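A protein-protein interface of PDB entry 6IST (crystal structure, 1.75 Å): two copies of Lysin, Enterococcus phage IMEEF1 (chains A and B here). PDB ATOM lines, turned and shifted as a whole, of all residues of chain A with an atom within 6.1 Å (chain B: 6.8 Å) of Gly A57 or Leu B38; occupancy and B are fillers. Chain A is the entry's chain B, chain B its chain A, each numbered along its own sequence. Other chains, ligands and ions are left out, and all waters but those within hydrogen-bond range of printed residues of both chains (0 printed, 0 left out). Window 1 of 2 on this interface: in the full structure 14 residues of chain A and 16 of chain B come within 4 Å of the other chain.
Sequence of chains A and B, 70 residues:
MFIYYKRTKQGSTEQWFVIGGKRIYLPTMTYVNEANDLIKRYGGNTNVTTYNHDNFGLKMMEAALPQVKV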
ATOM      1  N   TYR A  51      -2.417 -15.684  18.057  1.00  0.00           N
ATOM      2  CA  TYR A  51      -2.391 -16.427  19.252  1.00  0.00           C
ATOM      3  C   TYR A  51      -3.586 -16.068  20.132  1.00  0.00           C
ATOM      4  O   TYR A  51      -3.802 -14.920  20.408  1.00  0.00           O
ATOM      5  CB  TYR A  51      -1.109 -16.000  19.993  1.00  0.00           C
ATOM      6  CG  TYR A  51       0.138 -16.403  19.243  1.00  0.00           C
ATOM      7  CD1 TYR A  51       0.725 -15.573  18.317  1.00  0.00           C
ATOM      8  CD2 TYR A  51       0.718 -17.607  19.481  1.00  0.00           C
ATOM      9  CE1 TYR A  51       1.891 -15.939  17.646  1.00  0.00           C
ATOM     10  CE2 TYR A  51       1.893 -17.991  18.847  1.00  0.00           C
ATOM     11  CZ  TYR A  51       2.476 -17.150  17.917  1.00  0.00           C
ATOM     12  OH  TYR A  51       3.633 -17.524  17.262  1.00  0.00           O
ATOM     13  N   ASN A  55      -2.548 -19.114  24.934  1.00  0.00           N
ATOM     14  CA  ASN A  55      -1.569 -19.981  24.262  1.00  0.00           C
ATOM     15  C   ASN A  55      -0.200 -19.957  24.955  1.00  0.00           C
ATOM     16  O   ASN A  55       0.277 -18.894  25.294  1.00  0.00           O
ATOM     17  CB  ASN A  55      -1.409 -19.525  22.843  1.00  0.00           C
ATOM     18  CG  ASN A  55      -0.432 -20.359  22.082  1.00  0.00           C
ATOM     19  OD1 ASN A  55       0.776 -20.046  21.953  1.00  0.00           O
ATOM     20  ND2 ASN A  55      -0.928 -21.466  21.601  1.00  0.00           N
ATOM     21  N   PHE A  56       0.432 -21.126  25.152  1.00  0.00           N
ATOM     22  CA  PHE A  56       1.691 -21.216  25.887  1.00  0.00           C
ATOM     23  C   PHE A  56       2.867 -20.636  25.101  1.00  0.00           C
ATOM     24  O   PHE A  56       3.793 -20.085  25.661  1.00  0.00           O
ATOM     25  CB  PHE A  56       1.992 -22.678  26.259  1.00  0.00           C
ATOM     26  CG  PHE A  56       1.142 -23.220  27.377  1.00  0.00           C
ATOM     27  CD1 PHE A  56       0.184 -22.448  28.036  1.00  0.00           C
ATOM     28  CD2 PHE A  56       1.351 -24.515  27.814  1.00  0.00           C
ATOM     29  CE1 PHE A  56      -0.570 -22.988  29.070  1.00  0.00           C
ATOM     30  CE2 PHE A  56       0.598 -25.044  28.864  1.00  0.00           C
ATOM     31  CZ  PHE A  56      -0.353 -24.277  29.481  1.00  0.00           C
ATOM     32  N   GLY A  57       2.827 -20.745  23.788  1.00  0.00           N
ATOM     33  CA  GLY A  57       3.833 -20.103  22.957  1.00  0.00           C
ATOM     34  C   GLY A  57       3.794 -18.595  23.162  1.00  0.00           C
ATOM     35  O   GLY A  57       4.829 -17.978  23.410  1.00  0.00           O
ATOM     36  N   LEU A  58       2.596 -18.026  23.192  1.00  0.00           N
ATOM     37  CA  LEU A  58       2.439 -16.577  23.435  1.00  0.00           C
ATOM     38  C   LEU A  58       2.925 -16.210  24.816  1.00  0.00           C
ATOM     39  O   LEU A  58       3.658 -15.214  24.964  1.00  0.00           O
ATOM     40  CB  LEU A  58       0.991 -16.127  23.243  1.00  0.00           C
ATOM     41  CG  LEU A  58       0.661 -14.673  23.588  1.00  0.00           C
ATOM     42  CD1 LEU A  58       1.359 -13.777  22.573  1.00  0.00           C
ATOM     43  CD2 LEU A  58      -0.867 -14.398  23.612  1.00  0.00           C
ATOM     44  N   LYS A  59       2.492 -16.968  25.822  1.00  0.00           N
ATOM     45  CA  LYS A  59       3.008 -16.736  27.181  1.00  0.00           C
ATOM     46  C   LYS A  59       4.546 -16.774  27.304  1.00  0.00           C
ATOM     47  O   LYS A  59       5.108 -16.019  28.067  1.00  0.00           O
ATOM     48  CB  LYS A  59       2.414 -17.708  28.189  1.00  0.00           C
ATOM     49  CG  LYS A  59       0.907 -17.802  28.234  1.00  0.00           C
ATOM     50  CD  LYS A  59       0.272 -16.593  28.888  1.00  0.00           C
ATOM     51  CE  LYS A  59      -1.166 -16.926  29.302  1.00  0.00           C
ATOM     52  NZ  LYS A  59      -1.848 -15.726  29.835  1.00  0.00           N
ATOM     53  N   MET A  60       5.226 -17.638  26.554  1.00  0.00           N
ATOM     54  CA  MET A  60       6.697 -17.685  26.597  1.00  0.00           C
ATOM     55  C   MET A  60       7.254 -16.433  25.941  1.00  0.00           C
ATOM     56  O   MET A  60       8.157 -15.810  26.504  1.00  0.00           O
ATOM     57  CB  MET A  60       7.263 -19.001  25.983  1.00  0.00           C
ATOM     58  CG  MET A  60       6.949 -20.267  26.835  1.00  0.00           C
ATOM     59  SD  MET A  60       7.787 -21.771  26.257  1.00  0.00           S
ATOM     60  CE  MET A  60       6.774 -22.166  24.866  1.00  0.00           C
ATOM     61  N   MET A  61       6.714 -16.032  24.777  1.00  0.00           N
ATOM     62  CA  MET A  61       7.158 -14.799  24.146  1.00  0.00           C
ATOM     63  C   MET A  61       6.962 -13.615  25.090  1.00  0.00           C
ATOM     64  O   MET A  61       7.854 -12.776  25.211  1.00  0.00           O
ATOM     65  CB  MET A  61       6.434 -14.528  22.790  1.00  0.00           C
ATOM     66  CG  MET A  61       6.906 -15.429  21.678  1.00  0.00           C
ATOM     67  SD  MET A  61       6.391 -14.903  19.985  1.00  0.00           S
ATOM     68  CE  MET A  61       4.636 -15.188  20.123  1.00  0.00           C
ATOM     69  N   GLU A  62       5.832 -13.584  25.788  1.00  0.00           N
ATOM     70  CA  GLU A  62       5.477 -12.431  26.600  1.00  0.00           C
ATOM     71  C   GLU A  62       6.361 -12.370  27.826  1.00  0.00           C
ATOM     72  O   GLU A  62       6.716 -11.270  28.279  1.00  0.00           O
ATOM     73  CB  GLU A  62       3.978 -12.436  27.023  1.00  0.00           C
ATOM     74  CG  GLU A  62       3.074 -11.886  25.933  1.00  0.00           C
ATOM     75  CD  GLU A  62       1.560 -12.041  26.199  1.00  0.00           C
ATOM     76  OE1 GLU A  62       0.773 -11.328  25.542  1.00  0.00           O
ATOM     77  OE2 GLU A  62       1.131 -12.913  27.014  1.00  0.00           O
ATOM     78  N   MET B   1      16.600 -18.514  18.554  1.00  0.00           N
ATOM     79  CA  MET B   1      15.632 -19.408  19.169  1.00  0.00           C
ATOM     80  C   MET B   1      16.119 -20.820  18.961  1.00  0.00           C
ATOM     81  O   MET B   1      16.339 -21.201  17.830  1.00  0.00           O
ATOM     82  CB  MET B   1      14.310 -19.368  18.445  1.00  0.00           C
ATOM     83  CG  MET B   1      13.328 -18.313  18.883  1.00  0.00           C
ATOM     84  SD  MET B   1      11.699 -18.510  18.081  1.00  0.00           S
ATOM     85  CE  MET B   1      11.566 -20.196  18.250  1.00  0.00           C
ATOM     86  N   PHE B  17      14.535 -23.677  26.515  1.00  0.00           N
ATOM     87  CA  PHE B  17      14.162 -22.957  25.296  1.00  0.00           C
ATOM     88  C   PHE B  17      14.855 -21.619  25.348  1.00  0.00           C
ATOM     89  O   PHE B  17      14.693 -20.918  26.292  1.00  0.00           O
ATOM     90  CB  PHE B  17      12.647 -22.772  25.224  1.00  0.00           C
ATOM     91  CG  PHE B  17      12.148 -22.095  23.982  1.00  0.00           C
ATOM     92  CD1 PHE B  17      12.751 -22.288  22.748  1.00  0.00           C
ATOM     93  CD2 PHE B  17      11.087 -21.197  24.066  1.00  0.00           C
ATOM     94  CE1 PHE B  17      12.262 -21.669  21.632  1.00  0.00           C
ATOM     95  CE2 PHE B  17      10.579 -20.577  22.925  1.00  0.00           C
ATOM     96  CZ  PHE B  17      11.203 -20.782  21.720  1.00  0.00           C
ATOM     97  N   ILE B  19      15.184 -17.991  23.775  1.00  0.00           N
ATOM     98  CA  ILE B  19      14.391 -17.068  22.995  1.00  0.00           C
ATOM     99  C   ILE B  19      14.624 -15.677  23.520  1.00  0.00           C
ATOM    100  O   ILE B  19      14.735 -15.495  24.752  1.00  0.00           O
ATOM    101  CB  ILE B  19      12.880 -17.426  23.046  1.00  0.00           C
ATOM    102  CG1 ILE B  19      12.043 -16.394  22.251  1.00  0.00           C
ATOM    103  CG2 ILE B  19      12.385 -17.522  24.482  1.00  0.00           C
ATOM    104  CD1 ILE B  19      10.661 -16.841  21.824  1.00  0.00           C
ATOM    105  N   THR B  30       3.562 -29.985  26.664  1.00  0.00           N
ATOM    106  CA  THR B  30       2.801 -28.956  25.995  1.00  0.00           C
ATOM    107  C   THR B  30       3.644 -27.692  25.717  1.00  0.00           C
ATOM    108  O   THR B  30       3.567 -27.071  24.602  1.00  0.00           O
ATOM    109  CB  THR B  30       1.516 -28.608  26.772  1.00  0.00           C
ATOM    110  OG1 THR B  30       0.723 -29.804  26.922  1.00  0.00           O
ATOM    111  CG2 THR B  30       0.686 -27.586  25.963  1.00  0.00           C
ATOM    112  N   TYR B  31       4.451 -27.335  26.708  1.00  0.00           N
ATOM    113  CA  TYR B  31       5.421 -26.232  26.536  1.00  0.00           C
ATOM    114  C   TYR B  31       6.445 -26.559  25.481  1.00  0.00           C
ATOM    115  O   TYR B  31       6.756 -25.709  24.643  1.00  0.00           O
ATOM    116  CB  TYR B  31       6.108 -25.849  27.829  1.00  0.00           C
ATOM    117  CG  TYR B  31       5.192 -25.053  28.736  1.00  0.00           C
ATOM    118  CD1 TYR B  31       4.991 -23.713  28.524  1.00  0.00           C
ATOM    119  CD2 TYR B  31       4.544 -25.667  29.816  1.00  0.00           C
ATOM    120  CE1 TYR B  31       4.158 -22.957  29.354  1.00  0.00           C
ATOM    121  CE2 TYR B  31       3.717 -24.941  30.661  1.00  0.00           C
ATOM    122  CZ  TYR B  31       3.529 -23.592  30.447  1.00  0.00           C
ATOM    123  OH  TYR B  31       2.681 -22.878  31.284  1.00  0.00           O
ATOM    124  N   ASN B  33       6.183 -28.649  22.874  1.00  0.00           N
ATOM    125  CA  ASN B  33       5.495 -28.529  21.577  1.00  0.00           C
ATOM    126  C   ASN B  33       5.272 -27.083  21.071  1.00  0.00           C
ATOM    127  O   ASN B  33       5.513 -26.758  19.874  1.00  0.00           O
ATOM    128  CB  ASN B  33       4.176 -29.308  21.611  1.00  0.00           C
ATOM    129  CG  ASN B  33       4.404 -30.825  21.647  1.00  0.00           C
ATOM    130  OD1 ASN B  33       5.475 -31.331  21.280  1.00  0.00           O
ATOM    131  ND2 ASN B  33       3.379 -31.558  22.080  1.00  0.00           N
ATOM    132  N   GLU B  34       4.841 -26.224  21.976  1.00  0.00           N
ATOM    133  CA  GLU B  34       4.614 -24.831  21.639  1.00  0.00           C
ATOM    134  C   GLU B  34       5.958 -24.164  21.273  1.00  0.00           C
ATOM    135  O   GLU B  34       6.018 -23.422  20.287  1.00  0.00           O
ATOM    136  CB  GLU B  34       3.880 -24.092  22.758  1.00  0.00           C
ATOM    137  CG  GLU B  34       2.415 -24.574  22.903  1.00  0.00           C
ATOM    138  CD  GLU B  34       1.559 -24.363  21.655  1.00  0.00           C
ATOM    139  OE1 GLU B  34       1.811 -23.406  20.892  1.00  0.00           O
ATOM    140  OE2 GLU B  34       0.580 -25.120  21.445  1.00  0.00           O
ATOM    141  N   ALA B  35       7.027 -24.504  22.002  1.00  0.00           N
ATOM    142  CA  ALA B  35       8.369 -23.981  21.674  1.00  0.00           C
ATOM    143  C   ALA B  35       8.838 -24.398  20.294  1.00  0.00           C
ATOM    144  O   ALA B  35       9.303 -23.566  19.498  1.00  0.00           O
ATOM    145  CB  ALA B  35       9.380 -24.380  22.753  1.00  0.00           C
ATOM    146  N   ASN B  36       8.637 -25.678  19.961  1.00  0.00           N
ATOM    147  CA  ASN B  36       8.970 -26.124  18.648  1.00  0.00           C
ATOM    148  C   ASN B  36       8.163 -25.484  17.536  1.00  0.00           C
ATOM    149  O   ASN B  36       8.725 -25.278  16.428  1.00  0.00           O
ATOM    150  CB  ASN B  36       8.948 -27.661  18.535  1.00  0.00           C
ATOM    151  CG  ASN B  36      10.216 -28.291  19.129  1.00  0.00           C
ATOM    152  OD1 ASN B  36      11.334 -27.807  18.907  1.00  0.00           O
ATOM    153  ND2 ASN B  36      10.047 -29.303  19.918  1.00  0.00           N
ATOM    154  N   ASP B  37       6.883 -25.177  17.794  1.00  0.00           N
ATOM    155  CA  ASP B  37       6.056 -24.496  16.789  1.00  0.00           C
ATOM    156  C   ASP B  37       6.656 -23.077  16.603  1.00  0.00           C
ATOM    157  O   ASP B  37       6.690 -22.579  15.519  1.00  0.00           O
ATOM    158  CB  ASP B  37       4.578 -24.377  17.197  1.00  0.00           C
ATOM    159  CG  ASP B  37       3.823 -25.712  17.255  1.00  0.00           C
ATOM    160  OD1 ASP B  37       4.314 -26.728  16.699  1.00  0.00           O
ATOM    161  OD2 ASP B  37       2.710 -25.745  17.899  1.00  0.00           O
ATOM    162  N   LEU B  38       7.115 -22.448  17.681  1.00  0.00           N
ATOM    163  CA  LEU B  38       7.690 -21.131  17.574  1.00  0.00           C
ATOM    164  C   LEU B  38       8.978 -21.162  16.727  1.00  0.00           C
ATOM    165  O   LEU B  38       9.203 -20.282  15.830  1.00  0.00           O
ATOM    166  CB  LEU B  38       8.004 -20.519  18.934  1.00  0.00           C
ATOM    167  CG  LEU B  38       6.873 -20.021  19.858  1.00  0.00           C
ATOM    168  CD1 LEU B  38       7.497 -19.607  21.189  1.00  0.00           C
ATOM    169  CD2 LEU B  38       6.101 -18.905  19.220  1.00  0.00           C
ATOM    170  N   ILE B  39       9.809 -22.160  16.989  1.00  0.00           N
ATOM    171  CA  ILE B  39      11.005 -22.376  16.194  1.00  0.00           C
ATOM    172  C   ILE B  39      10.653 -22.475  14.761  1.00  0.00           C
ATOM    173  O   ILE B  39      11.325 -21.845  13.914  1.00  0.00           O
ATOM    174  CB  ILE B  39      11.835 -23.552  16.745  1.00  0.00           C
ATOM    175  CG1 ILE B  39      12.460 -23.169  18.109  1.00  0.00           C
ATOM    176  CG2 ILE B  39      12.951 -23.946  15.816  1.00  0.00           C
ATOM    177  CD1 ILE B  39      13.017 -24.346  18.868  1.00  0.00           C
ATOM    178  N   LYS B  40       9.684 -23.293  14.444  1.00  0.00           N
ATOM    179  CA  LYS B  40       9.345 -23.454  13.055  1.00  0.00           C
ATOM    180  C   LYS B  40       8.829 -22.183  12.409  1.00  0.00           C
ATOM    181  O   LYS B  40       9.153 -21.904  11.271  1.00  0.00           O
ATOM    182  CB  LYS B  40       8.326 -24.554  12.875  1.00  0.00           C
ATOM    183  CG  LYS B  40       8.217 -24.929  11.387  1.00  0.00           C
ATOM    184  CD  LYS B  40       7.282 -26.093  11.105  1.00  0.00           C
ATOM    185  CE  LYS B  40       7.854 -27.400  11.597  1.00  0.00           C
ATOM    186  NZ  LYS B  40       7.048 -28.520  11.036  1.00  0.00           N
ATOM    187  N   ARG B  41       7.974 -21.431  13.095  1.00  0.00           N
ATOM    188  CA  ARG B  41       7.391 -20.217  12.574  1.00  0.00           C
ATOM    189  C   ARG B  41       8.413 -19.142  12.289  1.00  0.00           C
ATOM    190  O   ARG B  41       8.357 -18.444  11.264  1.00  0.00           O
ATOM    191  CB  ARG B  41       6.374 -19.655  13.604  1.00  0.00           C
ATOM    192  CG  ARG B  41       5.080 -20.378  13.509  1.00  0.00           C
ATOM    193  CD  ARG B  41       3.887 -19.627  14.052  1.00  0.00           C
ATOM    194  NE  ARG B  41       3.779 -19.770  15.444  1.00  0.00           N
ATOM    195  CZ  ARG B  41       3.129 -20.719  16.094  1.00  0.00           C
ATOM    196  NH1 ARG B  41       2.457 -21.691  15.521  1.00  0.00           N
ATOM    197  NH2 ARG B  41       3.184 -20.659  17.401  1.00  0.00           N
ATOM    198  N   TYR B  42       9.315 -18.956  13.249  1.00  0.00           N
ATOM    199  CA  TYR B  42      10.184 -17.834  13.222  1.00  0.00           C
ATOM    200  C   TYR B  42      11.597 -18.152  12.769  1.00  0.00           C
ATOM    201  O   TYR B  42      12.482 -17.376  13.043  1.00  0.00           O
ATOM    202  CB  TYR B  42      10.139 -17.093  14.556  1.00  0.00           C
ATOM    203  CG  TYR B  42       8.708 -16.677  14.866  1.00  0.00           C
ATOM    204  CD1 TYR B  42       7.952 -15.904  13.951  1.00  0.00           C
ATOM    205  CD2 TYR B  42       8.080 -17.095  16.019  1.00  0.00           C
ATOM    206  CE1 TYR B  42       6.631 -15.535  14.211  1.00  0.00           C
ATOM    207  CE2 TYR B  42       6.760 -16.757  16.288  1.00  0.00           C
ATOM    208  CZ  TYR B  42       6.032 -15.961  15.387  1.00  0.00           C
ATOM    209  OH  TYR B  42       4.731 -15.644  15.659  1.00  0.00           O
ATOM    210  N   GLY B  43      11.800 -19.263  12.087  1.00  0.00           N
ATOM    211  CA  GLY B  43      13.125 -19.562  11.574  1.00  0.00           C
ATOM    212  C   GLY B  43      14.211 -19.825  12.607  1.00  0.00           C
ATOM    213  O   GLY B  43      15.349 -19.474  12.385  1.00  0.00           O
ATOM    214  N   GLY B  44      13.886 -20.500  13.695  1.00  0.00           N
ATOM    215  CA  GLY B  44      14.819 -20.794  14.716  1.00  0.00           C
ATOM    216  C   GLY B  44      15.682 -21.992  14.299  1.00  0.00           C
ATOM    217  O   GLY B  44      15.500 -22.593  13.253  1.00  0.00           O
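Gly A57 touches two residues of chain B.
Leu B38 touches just these residues of chain A: Tyr A51 and Gly A57.
Printed residues of chain A within 4 Å of Glu B34: Asn A55, Phe A56 and Gly A57.
Of the printed residues of chain B, Tyr A51 touches Leu B38 (3.4 Å), Arg B41 (2.9 Å) and Tyr B42 (2.7 Å).
Of the printed residues of chain A, Tyr B31 touches Phe A56 and Met A60.
Of the printed residues of chain A, Tyr B42 touches Tyr A51.
Gly B44 touches none of the printed residues of chain A.
The nearest residue of chain A that does not touch Leu B38 is Met A61 (4.1 Å).
The nearest printed residue of chain A that does not touch Arg B41 is Asn A55 (5.2 Å).
The side-chain amide oxygen (OD1) of Asn A55 lies within hydrogen-bond range of the backbone NH (N) of Gly A57 (2.8 Å).
The side-chain amide oxygen of Asn A55 lies within hydrogen-bond range of the backbone NH of Leu A58, at 3.0 Å.
Among the printed residues, pairs that only touch across the chains: Tyr A51 with Leu B38 (3.4 Å), Phe A56 with Tyr B31 (3.5 Å), Met A60 with Tyr B31 (3.6 Å), Phe A56 with Thr B30 (3.6 Å), Gly A57 with Glu B34 (3.7 Å), Met A60 with Ala B35 (3.7 Å), Gly A57 with Leu B38 (3.8 Å) and Phe A56 with Glu B34 (3.9 Å).
Along chain B the printed residues that touch a printed residue of chain A span positions 30 to 42.
No position is printed for both chains.
Of the 11 pairs that touch across the chains among the printed residues, none has its exchanged pair printed and touching as well.
OE1 of Glu B34 sits at hydrogen-bond distance from ND2 of Asn A55.
OH of Tyr A51 lies within hydrogen-bond range of NE of Arg B41, at 2.9 Å.
OH of Tyr B42 sits at hydrogen-bond distance from OH of Tyr A51 (2.7 Å).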
